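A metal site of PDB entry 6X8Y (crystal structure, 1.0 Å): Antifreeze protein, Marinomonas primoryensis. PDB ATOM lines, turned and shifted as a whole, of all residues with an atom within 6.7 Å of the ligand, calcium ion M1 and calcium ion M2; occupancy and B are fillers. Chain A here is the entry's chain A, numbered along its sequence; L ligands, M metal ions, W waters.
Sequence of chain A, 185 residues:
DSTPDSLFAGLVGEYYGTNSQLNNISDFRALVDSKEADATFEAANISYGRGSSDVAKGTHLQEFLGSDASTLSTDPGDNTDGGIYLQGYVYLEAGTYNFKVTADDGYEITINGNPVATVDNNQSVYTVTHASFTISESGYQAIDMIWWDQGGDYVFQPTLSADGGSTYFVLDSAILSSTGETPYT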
ATOM      1  N   ASN A  19     -33.579  -6.427 -29.911  1.00  0.00           N
ATOM      2  CA  ASN A  19     -32.978  -6.826 -31.182  1.00  0.00           C
ATOM      3  C   ASN A  19     -33.068  -5.773 -32.266  1.00  0.00           C
ATOM      4  O   ASN A  19     -32.779  -6.036 -33.445  1.00  0.00           O
ATOM      5  CB  ASN A  19     -33.551  -8.157 -31.658  1.00  0.00           C
ATOM      6  CG  ASN A  19     -33.314  -9.223 -30.607  1.00  0.00           C
ATOM      7  OD1 ASN A  19     -32.212  -9.313 -30.013  1.00  0.00           O
ATOM      8  ND2 ASN A  19     -34.311 -10.040 -30.327  1.00  0.00           N
ATOM      9  N   SER A  20     -33.490  -4.562 -31.870  1.00  0.00           N
ATOM     10  CA  SER A  20     -33.402  -3.372 -32.691  1.00  0.00           C
ATOM     11  C   SER A  20     -32.109  -2.623 -32.395  1.00  0.00           C
ATOM     12  O   SER A  20     -31.453  -2.868 -31.373  1.00  0.00           O
ATOM     13  CB  SER A  20     -34.619  -2.488 -32.417  1.00  0.00           C
ATOM     14  OG  SER A  20     -34.555  -1.878 -31.131  1.00  0.00           O
ATOM     15  N   GLN A  21     -31.735  -1.713 -33.304  1.00  0.00           N
ATOM     16  CA  GLN A  21     -30.503  -0.945 -33.148  1.00  0.00           C
ATOM     17  C   GLN A  21     -30.702   0.238 -32.204  1.00  0.00           C
ATOM     18  O   GLN A  21     -31.637   1.032 -32.342  1.00  0.00           O
ATOM     19  CB  GLN A  21     -30.050  -0.439 -34.518  1.00  0.00           C
ATOM     20  CG  GLN A  21     -28.978   0.621 -34.481  1.00  0.00           C
ATOM     21  CD  GLN A  21     -27.609   0.140 -33.986  1.00  0.00           C
ATOM     22  OE1 GLN A  21     -27.448  -0.986 -33.510  1.00  0.00           O
ATOM     23  NE2 GLN A  21     -26.593   0.999 -34.134  1.00  0.00           N
ATOM     24  N   LEU A  22     -29.770   0.383 -31.288  1.00  0.00           N
ATOM     25  CA  LEU A  22     -29.678   1.567 -30.424  1.00  0.00           C
ATOM     26  C   LEU A  22     -28.614   2.504 -30.999  1.00  0.00           C
ATOM     27  O   LEU A  22     -27.421   2.176 -30.968  1.00  0.00           O
ATOM     28  CB  LEU A  22     -29.328   1.143 -28.998  1.00  0.00           C
ATOM     29  CG  LEU A  22     -30.376   0.261 -28.298  1.00  0.00           C
ATOM     30  CD1 LEU A  22     -29.843  -0.199 -26.950  1.00  0.00           C
ATOM     31  CD2 LEU A  22     -31.728   0.955 -28.167  1.00  0.00           C
ATOM     32  N   GLY A  51     -15.830  -5.268 -21.525  1.00  0.00           N
ATOM     33  CA  GLY A  51     -15.916  -6.594 -22.128  1.00  0.00           C
ATOM     34  C   GLY A  51     -16.193  -6.480 -23.610  1.00  0.00           C
ATOM     35  O   GLY A  51     -16.282  -5.381 -24.176  1.00  0.00           O
ATOM     36  N   THR A  80     -29.396  -8.478 -29.189  1.00  0.00           N
ATOM     37  CA  THR A  80     -28.240  -7.901 -29.878  1.00  0.00           C
ATOM     38  C   THR A  80     -27.731  -6.621 -29.196  1.00  0.00           C
ATOM     39  O   THR A  80     -26.508  -6.371 -29.207  1.00  0.00           O
ATOM     40  CB  THR A  80     -28.561  -7.602 -31.358  1.00  0.00           C
ATOM     41  OG1 THR A  80     -29.562  -6.574 -31.468  1.00  0.00           O
ATOM     42  CG2 THR A  80     -29.082  -8.838 -32.076  1.00  0.00           C
ATOM     43  N   ASP A  81     -28.638  -5.842 -28.622  1.00  0.00           N
ATOM     44  CA  ASP A  81     -28.352  -4.527 -28.083  1.00  0.00           C
ATOM     45  C   ASP A  81     -28.952  -4.462 -26.684  1.00  0.00           C
ATOM     46  O   ASP A  81     -29.930  -5.159 -26.392  1.00  0.00           O
ATOM     47  CB  ASP A  81     -29.024  -3.428 -28.956  1.00  0.00           C
ATOM     48  CG  ASP A  81     -28.433  -3.262 -30.349  1.00  0.00           C
ATOM     49  OD1 ASP A  81     -28.274  -4.273 -31.073  1.00  0.00           O
ATOM     50  OD2 ASP A  81     -28.129  -2.102 -30.754  1.00  0.00           O
ATOM     51  N   ASP A 104     -18.428   2.967 -23.713  1.00  0.00           N
ATOM     52  CA  ASP A 104     -18.770   2.398 -25.032  1.00  0.00           C
ATOM     53  C   ASP A 104     -20.110   1.714 -24.740  1.00  0.00           C
ATOM     54  O   ASP A 104     -20.113   0.800 -23.897  1.00  0.00           O
ATOM     55  CB  ASP A 104     -17.691   1.434 -25.497  1.00  0.00           C
ATOM     56  CG  ASP A 104     -18.077   0.620 -26.708  1.00  0.00           C
ATOM     57  OD1 ASP A 104     -19.287   0.538 -27.055  1.00  0.00           O
ATOM     58  OD2 ASP A 104     -17.119   0.018 -27.337  1.00  0.00           O
ATOM     59  N   ASP A 105     -21.247   2.171 -25.271  1.00  0.00           N
ATOM     60  CA  ASP A 105     -21.458   3.230 -26.278  1.00  0.00           C
ATOM     61  C   ASP A 105     -21.740   4.552 -25.546  1.00  0.00           C
ATOM     62  O   ASP A 105     -20.854   5.043 -24.850  1.00  0.00           O
ATOM     63  CB  ASP A 105     -22.522   2.784 -27.286  1.00  0.00           C
ATOM     64  CG  ASP A 105     -21.954   1.786 -28.263  1.00  0.00           C
ATOM     65  OD1 ASP A 105     -21.234   2.249 -29.194  1.00  0.00           O
ATOM     66  OD2 ASP A 105     -22.141   0.545 -28.107  1.00  0.00           O
ATOM     67  N   ASN A 122     -23.221   6.382 -30.592  1.00  0.00           N
ATOM     68  CA  ASN A 122     -22.378   5.228 -30.403  1.00  0.00           C
ATOM     69  C   ASN A 122     -20.912   5.623 -30.494  1.00  0.00           C
ATOM     70  O   ASN A 122     -20.553   6.625 -31.108  1.00  0.00           O
ATOM     71  CB  ASN A 122     -22.733   4.118 -31.381  1.00  0.00           C
ATOM     72  CG  ASN A 122     -24.060   3.497 -31.061  1.00  0.00           C
ATOM     73  OD1 ASN A 122     -24.379   3.333 -29.887  1.00  0.00           O
ATOM     74  ND2 ASN A 122     -24.826   3.126 -32.081  1.00  0.00           N
ATOM     75  N   GLN A 123     -20.056   4.839 -29.821  1.00  0.00           N
ATOM     76  CA  GLN A 123     -18.617   5.097 -29.828  1.00  0.00           C
ATOM     77  C   GLN A 123     -17.868   3.905 -29.284  1.00  0.00           C
ATOM     78  O   GLN A 123     -18.311   3.281 -28.306  1.00  0.00           O
ATOM     79  CB  GLN A 123     -18.217   6.352 -29.004  1.00  0.00           C
ATOM     80  CG  GLN A 123     -18.699   6.300 -27.589  1.00  0.00           C
ATOM     81  CD  GLN A 123     -18.267   7.506 -26.760  1.00  0.00           C
ATOM     82  OE1 GLN A 123     -17.919   8.561 -27.295  1.00  0.00           O
ATOM     83  NE2 GLN A 123     -18.336   7.373 -25.462  1.00  0.00           N
ATOM     84  N   SER A 124     -16.703   3.610 -29.879  1.00  0.00           N
ATOM     85  CA  SER A 124     -15.745   2.785 -29.157  1.00  0.00           C
ATOM     86  C   SER A 124     -15.236   3.555 -27.927  1.00  0.00           C
ATOM     87  O   SER A 124     -15.417   4.769 -27.805  1.00  0.00           O
ATOM     88  CB  SER A 124     -14.608   2.369 -30.076  1.00  0.00           C
ATOM     89  OG  SER A 124     -14.008   3.458 -30.711  1.00  0.00           O
ATOM     90  N   VAL A 125     -14.572   2.843 -27.005  1.00  0.00           N
ATOM     91  CA  VAL A 125     -14.256   3.396 -25.693  1.00  0.00           C
ATOM     92  C   VAL A 125     -13.643   4.771 -25.808  1.00  0.00           C
ATOM     93  O   VAL A 125     -12.660   5.003 -26.523  1.00  0.00           O
ATOM     94  CB  VAL A 125     -13.374   2.449 -24.875  1.00  0.00           C
ATOM     95  CG1 VAL A 125     -12.087   2.110 -25.596  1.00  0.00           C
ATOM     96  CG2 VAL A 125     -13.088   3.043 -23.505  1.00  0.00           C
ATOM     97  N   TRP A 147     -27.213   4.228 -20.026  1.00  0.00           N
ATOM     98  CA  TRP A 147     -26.038   3.800 -20.783  1.00  0.00           C
ATOM     99  C   TRP A 147     -26.506   2.664 -21.687  1.00  0.00           C
ATOM    100  O   TRP A 147     -27.392   1.898 -21.283  1.00  0.00           O
ATOM    101  CB  TRP A 147     -24.909   3.305 -19.838  1.00  0.00           C
ATOM    102  CG  TRP A 147     -23.858   2.509 -20.569  1.00  0.00           C
ATOM    103  CD1 TRP A 147     -22.772   2.985 -21.235  1.00  0.00           C
ATOM    104  CD2 TRP A 147     -23.880   1.088 -20.815  1.00  0.00           C
ATOM    105  NE1 TRP A 147     -22.106   1.951 -21.857  1.00  0.00           N
ATOM    106  CE2 TRP A 147     -22.774   0.783 -21.628  1.00  0.00           C
ATOM    107  CE3 TRP A 147     -24.762   0.040 -20.456  1.00  0.00           C
ATOM    108  CZ2 TRP A 147     -22.511  -0.510 -22.097  1.00  0.00           C
ATOM    109  CZ3 TRP A 147     -24.490  -1.230 -20.931  1.00  0.00           C
ATOM    110  CH2 TRP A 147     -23.383  -1.491 -21.718  1.00  0.00           C
ATOM    111  N   TRP A 148     -25.917   2.538 -22.879  1.00  0.00           N
ATOM    112  CA  TRP A 148     -26.240   1.370 -23.678  1.00  0.00           C
ATOM    113  C   TRP A 148     -25.031   0.909 -24.482  1.00  0.00           C
ATOM    114  O   TRP A 148     -24.032   1.623 -24.631  1.00  0.00           O
ATOM    115  CB  TRP A 148     -27.439   1.670 -24.644  1.00  0.00           C
ATOM    116  CG  TRP A 148     -27.058   2.531 -25.819  1.00  0.00           C
ATOM    117  CD1 TRP A 148     -26.629   2.088 -27.032  1.00  0.00           C
ATOM    118  CD2 TRP A 148     -26.927   3.956 -25.857  1.00  0.00           C
ATOM    119  NE1 TRP A 148     -26.245   3.135 -27.841  1.00  0.00           N
ATOM    120  CE2 TRP A 148     -26.426   4.292 -27.135  1.00  0.00           C
ATOM    121  CE3 TRP A 148     -27.230   4.975 -24.944  1.00  0.00           C
ATOM    122  CZ2 TRP A 148     -26.169   5.609 -27.513  1.00  0.00           C
ATOM    123  CZ3 TRP A 148     -26.967   6.273 -25.331  1.00  0.00           C
ATOM    124  CH2 TRP A 148     -26.448   6.589 -26.589  1.00  0.00           C
ATOM    125  N   ASP A 149     -25.206  -0.296 -25.021  1.00  0.00           N
ATOM    126  CA  ASP A 149     -24.301  -0.945 -25.962  1.00  0.00           C
ATOM    127  C   ASP A 149     -25.101  -1.293 -27.219  1.00  0.00           C
ATOM    128  O   ASP A 149     -26.100  -2.025 -27.155  1.00  0.00           O
ATOM    129  CB  ASP A 149     -23.735  -2.234 -25.353  1.00  0.00           C
ATOM    130  CG  ASP A 149     -22.866  -2.996 -26.320  1.00  0.00           C
ATOM    131  OD1 ASP A 149     -22.160  -2.340 -27.112  1.00  0.00           O
ATOM    132  OD2 ASP A 149     -22.929  -4.254 -26.348  1.00  0.00           O
ATOM    133  N   GLN A 150     -24.641  -0.789 -28.369  1.00  0.00           N
ATOM    134  CA  GLN A 150     -25.214  -1.190 -29.670  1.00  0.00           C
ATOM    135  C   GLN A 150     -24.703  -2.545 -30.126  1.00  0.00           C
ATOM    136  O   GLN A 150     -25.211  -3.090 -31.120  1.00  0.00           O
ATOM    137  CB  GLN A 150     -24.920  -0.132 -30.755  1.00  0.00           C
ATOM    138  CG  GLN A 150     -23.449  -0.075 -31.168  1.00  0.00           C
ATOM    139  CD  GLN A 150     -23.195   0.324 -32.605  1.00  0.00           C
ATOM    140  OE1 GLN A 150     -23.972   0.028 -33.517  1.00  0.00           O
ATOM    141  NE2 GLN A 150     -22.052   0.995 -32.821  1.00  0.00           N
ATOM    142  N   GLY A 151     -23.678  -3.078 -29.459  1.00  0.00           N
ATOM    143  CA  GLY A 151     -22.984  -4.274 -29.868  1.00  0.00           C
ATOM    144  C   GLY A 151     -21.498  -4.090 -29.795  1.00  0.00           C
ATOM    145  O   GLY A 151     -20.967  -2.956 -29.731  1.00  0.00           O
ATOM    146  N   GLY A 152     -20.789  -5.207 -29.802  1.00  0.00           N
ATOM    147  CA  GLY A 152     -19.323  -5.199 -29.761  1.00  0.00           C
ATOM    148  C   GLY A 152     -18.790  -5.074 -28.364  1.00  0.00           C
ATOM    149  O   GLY A 152     -19.175  -5.850 -27.471  1.00  0.00           O
ATOM    150  N   ASP A 153     -17.874  -4.113 -28.162  1.00  0.00           N
ATOM    151  CA  ASP A 153     -17.316  -3.891 -26.852  1.00  0.00           C
ATOM    152  C   ASP A 153     -18.244  -2.994 -26.028  1.00  0.00           C
ATOM    153  O   ASP A 153     -19.187  -2.382 -26.540  1.00  0.00           O
ATOM    154  CB  ASP A 153     -15.903  -3.305 -26.992  1.00  0.00           C
ATOM    155  CG  ASP A 153     -14.924  -4.266 -27.699  1.00  0.00           C
ATOM    156  OD1 ASP A 153     -15.075  -5.492 -27.506  1.00  0.00           O
ATOM    157  OD2 ASP A 153     -14.004  -3.782 -28.381  1.00  0.00           O
ATOM    158  N   TYR A 154     -17.989  -2.938 -24.713  1.00  0.00           N
ATOM    159  CA  TYR A 154     -18.843  -2.210 -23.785  1.00  0.00           C
ATOM    160  C   TYR A 154     -18.066  -1.889 -22.529  1.00  0.00           C
ATOM    161  O   TYR A 154     -17.303  -2.716 -22.017  1.00  0.00           O
ATOM    162  CB  TYR A 154     -20.148  -3.008 -23.445  1.00  0.00           C
ATOM    163  CG  TYR A 154     -19.917  -4.488 -23.230  1.00  0.00           C
ATOM    164  CD1 TYR A 154     -19.939  -5.365 -24.313  1.00  0.00           C
ATOM    165  CD2 TYR A 154     -19.603  -4.993 -21.977  1.00  0.00           C
ATOM    166  CE1 TYR A 154     -19.655  -6.702 -24.146  1.00  0.00           C
ATOM    167  CE2 TYR A 154     -19.296  -6.346 -21.801  1.00  0.00           C
ATOM    168  CZ  TYR A 154     -19.300  -7.189 -22.900  1.00  0.00           C
ATOM    169  OH  TYR A 154     -18.945  -8.522 -22.712  1.00  0.00           O
ATOM    170  N   VAL A 155     -18.306  -0.685 -21.987  1.00  0.00           N
ATOM    171  CA  VAL A 155     -17.705  -0.254 -20.730  1.00  0.00           C
ATOM    172  C   VAL A 155     -18.504   0.950 -20.258  1.00  0.00           C
ATOM    173  O   VAL A 155     -19.006   1.731 -21.069  1.00  0.00           O
ATOM    174  CB  VAL A 155     -16.187   0.075 -20.875  1.00  0.00           C
ATOM    175  CG1 VAL A 155     -15.909   1.250 -21.813  1.00  0.00           C
ATOM    176  CG2 VAL A 155     -15.511   0.271 -19.503  1.00  0.00           C
HETATM  177  C1  LIG L   1     -18.222  -1.710 -31.565  1.00  0.00           C
HETATM  178  C2  LIG L   1     -17.906  -0.783 -30.413  1.00  0.00           C
HETATM  179  C3  LIG L   1     -18.714   0.489 -30.518  1.00  0.00           C
HETATM  180  C4  LIG L   1     -18.562   1.123 -31.881  1.00  0.00           C
HETATM  181  C5  LIG L   1     -18.818   0.088 -32.947  1.00  0.00           C
HETATM  182  O1  LIG L   1     -17.372  -2.829 -31.534  1.00  0.00           O
HETATM  183  O2  LIG L   1     -18.125  -1.445 -29.171  1.00  0.00           O
HETATM  184  O3  LIG L   1     -20.088   0.163 -30.245  1.00  0.00           O
HETATM  185  O4  LIG L   1     -19.483   2.190 -31.983  1.00  0.00           O
HETATM  186  O5  LIG L   1     -17.938  -1.002 -32.781  1.00  0.00           O
HETATM  187 CA    CA M   1     -20.435  -1.201 -28.174  1.00  0.00          CA
HETATM  188 CA    CA M   2     -26.932  -3.093 -32.712  1.00  0.00          CA
HETATM  189  O   HOH W   1     -18.468   4.004 -33.887  1.00  0.00           O
HETATM  190  O   HOH W   2     -26.082  -5.270 -33.342  1.00  0.00           O
HETATM  191  O   HOH W   3     -25.001  -2.561 -34.072  1.00  0.00           O
HETATM  192  O   HOH W   4     -28.527  -3.576 -34.316  1.00  0.00           O
HETATM  193  O   HOH W   5     -18.171  -4.675 -33.284  1.00  0.00           O
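The side-chain amide oxygen (OE1) of Gln 21 is bound to calcium ion M2, 2.3 Å away. Water W4 binds calcium ion M2, 2.3 Å away. The backbone carbonyl oxygen (O) of Gln 150 binds calcium ion M2. Water W2 binds calcium ion M2, at 2.4 Å. Calcium ion M2 is bound by water W3 (2.4 Å). Calcium ion M2 is bound by OD1 of Asp 81 (2.4 Å). Calcium ion M2 is bound by OD2 of Asp 81 (2.5 Å).
Calcium ion M1 is bound by the side-chain carboxylate of Asp 149, the side-chain carboxylate of Asp 104, the backbone carbonyl oxygen of Asp 153, the backbone carbonyl oxygen of Gly 151, the side-chain carboxylate of Asp 105, an oxygen (O3) of the ligand and an oxygen (O2) of the ligand.
Of the 22 residues printed, 5 come within 4 Å of calcium ion M1.
Asn 122 touches the ligand. N of Ser 124 touches C4 of the ligand, at 3.7 Å. Gly 152 touches the ligand.
O2 of the ligand sits close to N of Asp 153 (2.9 Å). NE2 of Gln 150 lies within hydrogen-bond range of O4 of the ligand, 3.0 Å away. The backbone NH (N) of Gln 123 is in hydrogen-bond range of an oxygen (O4) of the ligand (3.5 Å).
Of the 22 residues printed, 3 come within 4 Å of calcium ion M2.
NE1 of Trp 147 is in hydrogen-bond range of O of Asp 104 (3.1 Å). OD2 of Asp 81 lies close to N of Leu 22, 3.0 Å away. The side-chain carboxylate (OD1) of Asp 105 lies close to the side-chain amide oxygen (OD1) of Asn 122, at 3.4 Å. The side-chain amide nitrogen (NE2) of Gln 21 lies close to the side-chain amide nitrogen (ND2) of Asn 122 (3.4 Å). N of Asp 105 lies within hydrogen-bond range of O of Trp 148 (2.9 Å). OD1 of Asp 105 lies within hydrogen-bond range of N of Gln 123. N of Gln 150 sits close to OD2 of Asp 105 (2.8 Å). The side-chain carboxylate (OD1) of Asp 81 sits close to the side-chain hydroxyl (OG1) of Thr 80 (2.7 Å).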
